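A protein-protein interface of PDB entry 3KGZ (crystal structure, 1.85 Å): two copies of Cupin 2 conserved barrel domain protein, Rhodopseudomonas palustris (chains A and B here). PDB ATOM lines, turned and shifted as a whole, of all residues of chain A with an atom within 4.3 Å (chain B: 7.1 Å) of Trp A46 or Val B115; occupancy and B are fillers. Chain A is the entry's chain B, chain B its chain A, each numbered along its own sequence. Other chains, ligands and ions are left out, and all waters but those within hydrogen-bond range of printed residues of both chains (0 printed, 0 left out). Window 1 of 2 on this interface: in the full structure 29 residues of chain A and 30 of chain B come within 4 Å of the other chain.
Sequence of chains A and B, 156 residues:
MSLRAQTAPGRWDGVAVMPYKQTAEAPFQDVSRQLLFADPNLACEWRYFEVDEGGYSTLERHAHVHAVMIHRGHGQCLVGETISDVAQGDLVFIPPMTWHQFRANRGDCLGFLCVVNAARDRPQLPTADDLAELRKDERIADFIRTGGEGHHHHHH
Trp A46 touches just these residues of chain B: Ala B67, Met B69 and Val B115. Val B115 touches one residue of chain A. Printed residues of chain B within 4 Å of Val A115: Trp B46 (3.4 Å). Of the printed residues of chain B, Phe A37 touches Ala B67 (3.5 Å), Val B68 (3.3 Å), Leu B91 (3.9 Å) and Val B92 (3.5 Å). Printed residues of chain A within 4 Å of Val B65: Leu A42 (3.96 Å). His B66 touches none of the printed residues of chain A. His B64 touches none of the printed residues of chain A. The nearest residue of chain A that does not touch Val B115 is Leu A42 (4.2 Å).
Trp A46 touches Val B115, and with the chains exchanged Val A115 touches Trp B46. Leu A113 touches its own counterpart, Leu B113. Positions printed for both chains: 45, 46, 47, 113, 114 and 115.
Among the printed residues, pairs that only touch across the chains: Leu A36 with Met B69 (3.7 Å), Phe A37 with Ala B67 (3.5 Å), Phe A37 with Val B68 (3.3 Å), Phe A37 with Leu B91 (3.9 Å), Phe A37 with Val B92 (3.5 Å), Leu A42 with Val B65 (3.96 Å), Leu A42 with Asn B117 (3.6 Å), Trp A46 with Ala B67 (3.5 Å), Trp A46 with Met B69 (3.5 Å), Trp A46 with Val B115 (3.5 Å), Leu A113 with Met B69 (3.7 Å), Leu A113 with Leu B113 (3.96 Å) and Val A115 with Trp B46 (3.4 Å).
Hydrophobic or aromatic side chains of chain A that line the printed part of chain B: Leu A36, Phe A37, Leu A42, Trp A46, Leu A113 and Val A115. Of the 19 printed residues of chain B, 10 touch a printed residue of chain A. Among the printed residues, 13 pairs touch across the chains. Among the printed residues, no Asp or Glu carboxylate lies within 4 Å of a Lys or Arg side-chain nitrogen of the other chain.
The side-chain sulfur (SG) of Cys B44 sits at hydrogen-bond distance from the side-chain amide oxygen (OD1) of Asn B117 (3.4 Å). The backbone carbonyl oxygen (O) of Ala B67 is in hydrogen-bond range of the backbone NH (N) of Val B115 (2.8 Å). The backbone carbonyl oxygen (O) of Val B68 sits at hydrogen-bond distance from the backbone NH (N) of Val B92, at 2.8 Å. N of Leu B113 is in hydrogen-bond range of O of Met B69, at 2.8 Å. N of Leu A36 sits at hydrogen-bond distance from O of Trp A46 (2.9 Å). The backbone NH (N) of Trp A46 is in hydrogen-bond range of the backbone carbonyl oxygen (O) of Phe A37, at 3.0 Å.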
ATOM      1  N   LEU A  35      35.101 -24.926  -7.007  1.00  0.00           N
ATOM      2  CA  LEU A  35      34.016 -24.747  -7.972  1.00  0.00           C
ATOM      3  C   LEU A  35      32.737 -24.453  -7.260  1.00  0.00           C
ATOM      4  O   LEU A  35      32.199 -25.301  -6.522  1.00  0.00           O
ATOM      5  CB  LEU A  35      33.869 -25.983  -8.853  1.00  0.00           C
ATOM      6  CG  LEU A  35      32.823 -25.796  -9.962  1.00  0.00           C
ATOM      7  CD1 LEU A  35      33.219 -24.682 -10.918  1.00  0.00           C
ATOM      8  CD2 LEU A  35      32.719 -27.148 -10.689  1.00  0.00           C
ATOM      9  N   LEU A  36      32.263 -23.223  -7.403  1.00  0.00           N
ATOM     10  CA  LEU A  36      31.075 -22.796  -6.644  1.00  0.00           C
ATOM     11  C   LEU A  36      29.815 -23.139  -7.450  1.00  0.00           C
ATOM     12  O   LEU A  36      28.882 -23.707  -6.909  1.00  0.00           O
ATOM     13  CB  LEU A  36      31.141 -21.325  -6.348  1.00  0.00           C
ATOM     14  CG  LEU A  36      32.429 -20.875  -5.644  1.00  0.00           C
ATOM     15  CD1 LEU A  36      32.323 -19.402  -5.232  1.00  0.00           C
ATOM     16  CD2 LEU A  36      32.742 -21.774  -4.429  1.00  0.00           C
ATOM     17  N   PHE A  37      29.798 -22.792  -8.740  1.00  0.00           N
ATOM     18  CA  PHE A  37      28.590 -23.126  -9.571  1.00  0.00           C
ATOM     19  C   PHE A  37      29.015 -23.559 -10.964  1.00  0.00           C
ATOM     20  O   PHE A  37      29.793 -22.843 -11.616  1.00  0.00           O
ATOM     21  CB  PHE A  37      27.706 -21.917  -9.749  1.00  0.00           C
ATOM     22  CG  PHE A  37      27.077 -21.391  -8.478  1.00  0.00           C
ATOM     23  CD1 PHE A  37      25.864 -21.900  -8.043  1.00  0.00           C
ATOM     24  CD2 PHE A  37      27.671 -20.383  -7.749  1.00  0.00           C
ATOM     25  CE1 PHE A  37      25.253 -21.405  -6.915  1.00  0.00           C
ATOM     26  CE2 PHE A  37      27.053 -19.907  -6.579  1.00  0.00           C
ATOM     27  CZ  PHE A  37      25.830 -20.427  -6.197  1.00  0.00           C
ATOM     28  N   LEU A  42      23.597 -23.163 -17.091  1.00  0.00           N
ATOM     29  CA  LEU A  42      24.286 -21.908 -16.812  1.00  0.00           C
ATOM     30  C   LEU A  42      25.419 -21.767 -17.787  1.00  0.00           C
ATOM     31  O   LEU A  42      26.268 -22.657 -17.916  1.00  0.00           O
ATOM     32  CB  LEU A  42      24.781 -21.910 -15.353  1.00  0.00           C
ATOM     33  CG  LEU A  42      25.158 -20.586 -14.699  1.00  0.00           C
ATOM     34  CD1 LEU A  42      24.013 -19.584 -14.574  1.00  0.00           C
ATOM     35  CD2 LEU A  42      25.775 -20.867 -13.293  1.00  0.00           C
ATOM     36  N   GLU A  45      30.753 -20.475 -15.558  1.00  0.00           N
ATOM     37  CA  GLU A  45      31.163 -21.194 -14.353  1.00  0.00           C
ATOM     38  C   GLU A  45      31.683 -20.161 -13.384  1.00  0.00           C
ATOM     39  O   GLU A  45      32.228 -19.151 -13.799  1.00  0.00           O
ATOM     40  CB  GLU A  45      32.225 -22.203 -14.652  1.00  0.00           C
ATOM     41  CG  GLU A  45      31.712 -23.271 -15.621  1.00  0.00           C
ATOM     42  CD  GLU A  45      32.780 -24.035 -16.377  1.00  0.00           C
ATOM     43  OE1 GLU A  45      33.987 -23.695 -16.348  1.00  0.00           O
ATOM     44  OE2 GLU A  45      32.364 -25.017 -17.023  1.00  0.00           O
ATOM     45  N   TRP A  46      31.474 -20.411 -12.111  1.00  0.00           N
ATOM     46  CA  TRP A  46      31.804 -19.452 -11.066  1.00  0.00           C
ATOM     47  C   TRP A  46      32.727 -20.197 -10.120  1.00  0.00           C
ATOM     48  O   TRP A  46      32.340 -21.219  -9.524  1.00  0.00           O
ATOM     49  CB  TRP A  46      30.497 -19.045 -10.387  1.00  0.00           C
ATOM     50  CG  TRP A  46      30.564 -18.022  -9.317  1.00  0.00           C
ATOM     51  CD1 TRP A  46      31.658 -17.578  -8.621  1.00  0.00           C
ATOM     52  CD2 TRP A  46      29.444 -17.301  -8.796  1.00  0.00           C
ATOM     53  NE1 TRP A  46      31.278 -16.622  -7.706  1.00  0.00           N
ATOM     54  CE2 TRP A  46      29.927 -16.432  -7.796  1.00  0.00           C
ATOM     55  CE3 TRP A  46      28.086 -17.322  -9.071  1.00  0.00           C
ATOM     56  CZ2 TRP A  46      29.084 -15.588  -7.086  1.00  0.00           C
ATOM     57  CZ3 TRP A  46      27.267 -16.500  -8.400  1.00  0.00           C
ATOM     58  CH2 TRP A  46      27.750 -15.638  -7.407  1.00  0.00           C
ATOM     59  N   ARG A  47      33.957 -19.718 -10.014  1.00  0.00           N
ATOM     60  CA  ARG A  47      34.966 -20.361  -9.178  1.00  0.00           C
ATOM     61  C   ARG A  47      35.465 -19.388  -8.102  1.00  0.00           C
ATOM     62  O   ARG A  47      35.200 -18.195  -8.145  1.00  0.00           O
ATOM     63  CB  ARG A  47      36.152 -20.848 -10.001  1.00  0.00           C
ATOM     64  CG  ARG A  47      35.861 -22.100 -10.818  1.00  0.00           C
ATOM     65  CD  ARG A  47      37.055 -22.488 -11.664  1.00  0.00           C
ATOM     66  NE  ARG A  47      36.725 -23.686 -12.395  1.00  0.00           N
ATOM     67  CZ  ARG A  47      36.095 -23.689 -13.570  1.00  0.00           C
ATOM     68  NH1 ARG A  47      35.792 -22.550 -14.161  1.00  0.00           N
ATOM     69  NH2 ARG A  47      35.785 -24.835 -14.155  1.00  0.00           N
ATOM     70  N   LEU A 113      36.581 -14.420  -6.417  1.00  0.00           N
ATOM     71  CA  LEU A 113      35.567 -15.075  -7.260  1.00  0.00           C
ATOM     72  C   LEU A 113      35.930 -14.808  -8.675  1.00  0.00           C
ATOM     73  O   LEU A 113      36.360 -13.692  -9.023  1.00  0.00           O
ATOM     74  CB  LEU A 113      34.180 -14.468  -6.968  1.00  0.00           C
ATOM     75  CG  LEU A 113      33.731 -14.452  -5.483  1.00  0.00           C
ATOM     76  CD1 LEU A 113      32.336 -13.868  -5.391  1.00  0.00           C
ATOM     77  CD2 LEU A 113      33.781 -15.882  -4.868  1.00  0.00           C
ATOM     78  N   CYS A 114      35.688 -15.785  -9.545  1.00  0.00           N
ATOM     79  CA  CYS A 114      35.999 -15.622 -10.952  1.00  0.00           C
ATOM     80  C   CYS A 114      34.866 -16.264 -11.761  1.00  0.00           C
ATOM     81  O   CYS A 114      34.555 -17.420 -11.518  1.00  0.00           O
ATOM     82  CB  CYS A 114      37.305 -16.323 -11.256  1.00  0.00           C
ATOM     83  SG  CYS A 114      37.861 -16.141 -13.006  1.00  0.00           S
ATOM     84  N   VAL A 115      34.249 -15.488 -12.632  1.00  0.00           N
ATOM     85  CA  VAL A 115      33.182 -15.971 -13.522  1.00  0.00           C
ATOM     86  C   VAL A 115      33.708 -15.896 -14.943  1.00  0.00           C
ATOM     87  O   VAL A 115      34.189 -14.830 -15.393  1.00  0.00           O
ATOM     88  CB  VAL A 115      31.922 -15.184 -13.322  1.00  0.00           C
ATOM     89  CG1 VAL A 115      30.843 -15.528 -14.367  1.00  0.00           C
ATOM     90  CG2 VAL A 115      31.357 -15.433 -11.899  1.00  0.00           C
ATOM     91  N   CYS B  44      26.918 -14.469 -19.189  1.00  0.00           N
ATOM     92  CA  CYS B  44      26.021 -14.234 -18.062  1.00  0.00           C
ATOM     93  C   CYS B  44      26.072 -12.770 -17.606  1.00  0.00           C
ATOM     94  O   CYS B  44      26.972 -12.021 -18.014  1.00  0.00           O
ATOM     95  CB  CYS B  44      26.373 -15.155 -16.883  1.00  0.00           C
ATOM     96  SG  CYS B  44      25.943 -16.964 -17.088  1.00  0.00           S
ATOM     97  N   GLU B  45      25.086 -12.363 -16.802  1.00  0.00           N
ATOM     98  CA  GLU B  45      25.033 -11.044 -16.162  1.00  0.00           C
ATOM     99  C   GLU B  45      25.161 -11.257 -14.639  1.00  0.00           C
ATOM    100  O   GLU B  45      24.604 -12.184 -14.087  1.00  0.00           O
ATOM    101  CB  GLU B  45      23.726 -10.300 -16.478  1.00  0.00           C
ATOM    102  CG  GLU B  45      23.593 -10.029 -17.998  1.00  0.00           C
ATOM    103  CD  GLU B  45      22.294  -9.440 -18.443  1.00  0.00           C
ATOM    104  OE1 GLU B  45      21.246  -9.609 -17.790  1.00  0.00           O
ATOM    105  OE2 GLU B  45      22.335  -8.816 -19.527  1.00  0.00           O
ATOM    106  N   TRP B  46      25.938 -10.403 -13.998  1.00  0.00           N
ATOM    107  CA  TRP B  46      26.220 -10.568 -12.565  1.00  0.00           C
ATOM    108  C   TRP B  46      25.714  -9.274 -11.915  1.00  0.00           C
ATOM    109  O   TRP B  46      26.146  -8.187 -12.271  1.00  0.00           O
ATOM    110  CB  TRP B  46      27.705 -10.750 -12.424  1.00  0.00           C
ATOM    111  CG  TRP B  46      28.250 -11.016 -11.082  1.00  0.00           C
ATOM    112  CD1 TRP B  46      27.636 -10.854  -9.885  1.00  0.00           C
ATOM    113  CD2 TRP B  46      29.576 -11.464 -10.808  1.00  0.00           C
ATOM    114  NE1 TRP B  46      28.508 -11.200  -8.862  1.00  0.00           N
ATOM    115  CE2 TRP B  46      29.711 -11.555  -9.409  1.00  0.00           C
ATOM    116  CE3 TRP B  46      30.674 -11.780 -11.615  1.00  0.00           C
ATOM    117  CZ2 TRP B  46      30.905 -11.984  -8.798  1.00  0.00           C
ATOM    118  CZ3 TRP B  46      31.857 -12.194 -11.022  1.00  0.00           C
ATOM    119  CH2 TRP B  46      31.959 -12.309  -9.622  1.00  0.00           C
ATOM    120  N   ARG B  47      24.745  -9.408 -11.032  1.00  0.00           N
ATOM    121  CA  ARG B  47      24.138  -8.305 -10.351  1.00  0.00           C
ATOM    122  C   ARG B  47      24.263  -8.487  -8.850  1.00  0.00           C
ATOM    123  O   ARG B  47      24.594  -9.573  -8.345  1.00  0.00           O
ATOM    124  CB  ARG B  47      22.660  -8.238 -10.713  1.00  0.00           C
ATOM    125  CG  ARG B  47      22.389  -7.753 -12.121  1.00  0.00           C
ATOM    126  CD  ARG B  47      20.885  -7.676 -12.431  1.00  0.00           C
ATOM    127  NE  ARG B  47      20.639  -7.183 -13.795  1.00  0.00           N
ATOM    128  CZ  ARG B  47      20.695  -7.946 -14.888  1.00  0.00           C
ATOM    129  NH1 ARG B  47      20.972  -9.233 -14.804  1.00  0.00           N
ATOM    130  NH2 ARG B  47      20.478  -7.416 -16.075  1.00  0.00           N
ATOM    131  N   PHE B  49      21.764  -7.581  -5.581  1.00  0.00           N
ATOM    132  CA  PHE B  49      20.413  -7.216  -5.220  1.00  0.00           C
ATOM    133  C   PHE B  49      20.478  -6.932  -3.749  1.00  0.00           C
ATOM    134  O   PHE B  49      21.158  -7.666  -3.012  1.00  0.00           O
ATOM    135  CB  PHE B  49      19.462  -8.353  -5.471  1.00  0.00           C
ATOM    136  CG  PHE B  49      19.090  -8.520  -6.917  1.00  0.00           C
ATOM    137  CD1 PHE B  49      18.114  -7.716  -7.493  1.00  0.00           C
ATOM    138  CD2 PHE B  49      19.696  -9.487  -7.695  1.00  0.00           C
ATOM    139  CE1 PHE B  49      17.762  -7.870  -8.831  1.00  0.00           C
ATOM    140  CE2 PHE B  49      19.347  -9.647  -9.039  1.00  0.00           C
ATOM    141  CZ  PHE B  49      18.379  -8.831  -9.607  1.00  0.00           C
ATOM    142  N   HIS B  64      15.025 -20.298 -16.525  1.00  0.00           N
ATOM    143  CA  HIS B  64      16.428 -19.965 -16.297  1.00  0.00           C
ATOM    144  C   HIS B  64      16.813 -20.159 -14.818  1.00  0.00           C
ATOM    145  O   HIS B  64      16.012 -19.921 -13.907  1.00  0.00           O
ATOM    146  CB  HIS B  64      16.775 -18.575 -16.842  1.00  0.00           C
ATOM    147  CG  HIS B  64      16.320 -17.409 -15.998  1.00  0.00           C
ATOM    148  ND1 HIS B  64      15.221 -16.640 -16.312  1.00  0.00           N
ATOM    149  CD2 HIS B  64      16.891 -16.819 -14.917  1.00  0.00           C
ATOM    150  CE1 HIS B  64      15.116 -15.643 -15.439  1.00  0.00           C
ATOM    151  NE2 HIS B  64      16.126 -15.730 -14.586  1.00  0.00           N
ATOM    152  N   VAL B  65      18.061 -20.602 -14.591  1.00  0.00           N
ATOM    153  CA  VAL B  65      18.534 -20.869 -13.220  1.00  0.00           C
ATOM    154  C   VAL B  65      19.192 -19.619 -12.607  1.00  0.00           C
ATOM    155  O   VAL B  65      19.568 -18.690 -13.332  1.00  0.00           O
ATOM    156  CB  VAL B  65      19.515 -22.104 -13.165  1.00  0.00           C
ATOM    157  CG1 VAL B  65      18.816 -23.417 -13.737  1.00  0.00           C
ATOM    158  CG2 VAL B  65      20.823 -21.836 -13.897  1.00  0.00           C
ATOM    159  N   HIS B  66      19.299 -19.609 -11.272  1.00  0.00           N
ATOM    160  CA  HIS B  66      20.016 -18.580 -10.537  1.00  0.00           C
ATOM    161  C   HIS B  66      21.179 -19.194  -9.744  1.00  0.00           C
ATOM    162  O   HIS B  66      20.975 -20.171  -9.035  1.00  0.00           O
ATOM    163  CB  HIS B  66      19.152 -17.969  -9.449  1.00  0.00           C
ATOM    164  CG  HIS B  66      18.173 -16.944  -9.915  1.00  0.00           C
ATOM    165  ND1 HIS B  66      18.547 -15.732 -10.458  1.00  0.00           N
ATOM    166  CD2 HIS B  66      16.822 -16.902  -9.803  1.00  0.00           C
ATOM    167  CE1 HIS B  66      17.463 -15.018 -10.725  1.00  0.00           C
ATOM    168  NE2 HIS B  66      16.405 -15.712 -10.345  1.00  0.00           N
ATOM    169  N   ALA B  67      22.332 -18.562  -9.837  1.00  0.00           N
ATOM    170  CA  ALA B  67      23.446 -18.813  -8.938  1.00  0.00           C
ATOM    171  C   ALA B  67      23.545 -17.591  -8.046  1.00  0.00           C
ATOM    172  O   ALA B  67      23.724 -16.463  -8.514  1.00  0.00           O
ATOM    173  CB  ALA B  67      24.752 -19.051  -9.715  1.00  0.00           C
ATOM    174  N   VAL B  68      23.335 -17.824  -6.751  1.00  0.00           N
ATOM    175  CA  VAL B  68      23.287 -16.753  -5.729  1.00  0.00           C
ATOM    176  C   VAL B  68      24.329 -16.969  -4.633  1.00  0.00           C
ATOM    177  O   VAL B  68      24.537 -18.104  -4.176  1.00  0.00           O
ATOM    178  CB  VAL B  68      21.893 -16.645  -5.122  1.00  0.00           C
ATOM    179  CG1 VAL B  68      21.867 -15.646  -3.940  1.00  0.00           C
ATOM    180  CG2 VAL B  68      20.918 -16.151  -6.182  1.00  0.00           C
ATOM    181  N   MET B  69      25.006 -15.887  -4.262  1.00  0.00           N
ATOM    182  CA  MET B  69      25.923 -15.860  -3.133  1.00  0.00           C
ATOM    183  C   MET B  69      25.531 -14.690  -2.250  1.00  0.00           C
ATOM    184  O   MET B  69      25.443 -13.549  -2.683  1.00  0.00           O
ATOM    185  CB  MET B  69      27.400 -15.752  -3.553  1.00  0.00           C
ATOM    186  CG  MET B  69      28.347 -15.829  -2.339  1.00  0.00           C
ATOM    187  SD  MET B  69      30.127 -15.599  -2.729  1.00  0.00           S
ATOM    188  CE  MET B  69      30.275 -16.660  -3.948  1.00  0.00           C
ATOM    189  N   ILE B  70      25.228 -14.991  -0.993  1.00  0.00           N
ATOM    190  CA  ILE B  70      24.897 -13.924  -0.064  1.00  0.00           C
ATOM    191  C   ILE B  70      26.119 -13.023   0.172  1.00  0.00           C
ATOM    192  O   ILE B  70      27.244 -13.481   0.449  1.00  0.00           O
ATOM    193  CB  ILE B  70      24.296 -14.453   1.255  1.00  0.00           C
ATOM    194  CG1 ILE B  70      23.179 -15.462   1.014  1.00  0.00           C
ATOM    195  CG2 ILE B  70      23.854 -13.259   2.121  1.00  0.00           C
ATOM    196  CD1 ILE B  70      21.985 -14.976   0.136  1.00  0.00           C
ATOM    197  N   LEU B  91      25.899 -20.087  -0.493  1.00  0.00           N
ATOM    198  CA  LEU B  91      25.645 -20.312  -1.913  1.00  0.00           C
ATOM    199  C   LEU B  91      24.263 -20.901  -2.064  1.00  0.00           C
ATOM    200  O   LEU B  91      23.968 -21.937  -1.470  1.00  0.00           O
ATOM    201  CB  LEU B  91      26.657 -21.297  -2.473  1.00  0.00           C
ATOM    202  CG  LEU B  91      28.113 -20.990  -2.169  1.00  0.00           C
ATOM    203  CD1 LEU B  91      29.014 -22.142  -2.643  1.00  0.00           C
ATOM    204  CD2 LEU B  91      28.501 -19.624  -2.804  1.00  0.00           C
ATOM    205  N   VAL B  92      23.429 -20.292  -2.886  1.00  0.00           N
ATOM    206  CA  VAL B  92      22.115 -20.825  -3.184  1.00  0.00           C
ATOM    207  C   VAL B  92      22.014 -21.046  -4.701  1.00  0.00           C
ATOM    208  O   VAL B  92      22.305 -20.156  -5.486  1.00  0.00           O
ATOM    209  CB  VAL B  92      20.997 -19.866  -2.743  1.00  0.00           C
ATOM    210  CG1 VAL B  92      19.607 -20.376  -3.198  1.00  0.00           C
ATOM    211  CG2 VAL B  92      21.009 -19.665  -1.217  1.00  0.00           C
ATOM    212  N   LEU B 113      24.599 -11.530  -4.400  1.00  0.00           N
ATOM    213  CA  LEU B 113      25.101 -11.575  -5.769  1.00  0.00           C
ATOM    214  C   LEU B 113      24.217 -12.553  -6.507  1.00  0.00           C
ATOM    215  O   LEU B 113      23.855 -13.593  -5.969  1.00  0.00           O
ATOM    216  CB  LEU B 113      26.540 -12.068  -5.802  1.00  0.00           C
ATOM    217  CG  LEU B 113      27.505 -11.328  -4.862  1.00  0.00           C
ATOM    218  CD1 LEU B 113      28.891 -11.986  -4.874  1.00  0.00           C
ATOM    219  CD2 LEU B 113      27.592  -9.862  -5.240  1.00  0.00           C
ATOM    220  N   CYS B 114      23.917 -12.251  -7.773  1.00  0.00           N
ATOM    221  CA  CYS B 114      23.065 -13.109  -8.553  1.00  0.00           C
ATOM    222  C   CYS B 114      23.662 -13.176  -9.959  1.00  0.00           C
ATOM    223  O   CYS B 114      23.849 -12.121 -10.559  1.00  0.00           O
ATOM    224  CB  CYS B 114      21.675 -12.498  -8.609  1.00  0.00           C
ATOM    225  SG  CYS B 114      20.514 -13.613  -9.391  1.00  0.00           S
ATOM    226  N   VAL B 115      23.983 -14.378 -10.425  1.00  0.00           N
ATOM    227  CA  VAL B 115      24.489 -14.635 -11.751  1.00  0.00           C
ATOM    228  C   VAL B 115      23.410 -15.410 -12.551  1.00  0.00           C
ATOM    229  O   VAL B 115      22.881 -16.417 -12.090  1.00  0.00           O
ATOM    230  CB  VAL B 115      25.835 -15.370 -11.716  1.00  0.00           C
ATOM    231  CG1 VAL B 115      26.250 -15.829 -13.062  1.00  0.00           C
ATOM    232  CG2 VAL B 115      26.934 -14.419 -11.174  1.00  0.00           C
ATOM    233  N   VAL B 116      23.077 -14.896 -13.735  1.00  0.00           N
ATOM    234  CA  VAL B 116      22.071 -15.528 -14.626  1.00  0.00           C
ATOM    235  C   VAL B 116      22.539 -15.399 -16.068  1.00  0.00           C
ATOM    236  O   VAL B 116      23.320 -14.525 -16.409  1.00  0.00           O
ATOM    237  CB  VAL B 116      20.694 -14.871 -14.539  1.00  0.00           C
ATOM    238  CG1 VAL B 116      20.042 -15.061 -13.176  1.00  0.00           C
ATOM    239  CG2 VAL B 116      20.777 -13.366 -14.865  1.00  0.00           C
ATOM    240  N   ASN B 117      22.024 -16.262 -16.939  1.00  0.00           N
ATOM    241  CA  ASN B 117      22.366 -16.159 -18.368  1.00  0.00           C
ATOM    242  C   ASN B 117      21.942 -14.828 -18.957  1.00  0.00           C
ATOM    243  O   ASN B 117      20.885 -14.304 -18.600  1.00  0.00           O
ATOM    244  CB  ASN B 117      21.673 -17.262 -19.155  1.00  0.00           C
ATOM    245  CG  ASN B 117      22.283 -18.612 -18.921  1.00  0.00           C
ATOM    246  OD1 ASN B 117      23.347 -18.734 -18.304  1.00  0.00           O
ATOM    247  ND2 ASN B 117      21.592 -19.659 -19.394  1.00  0.00           N
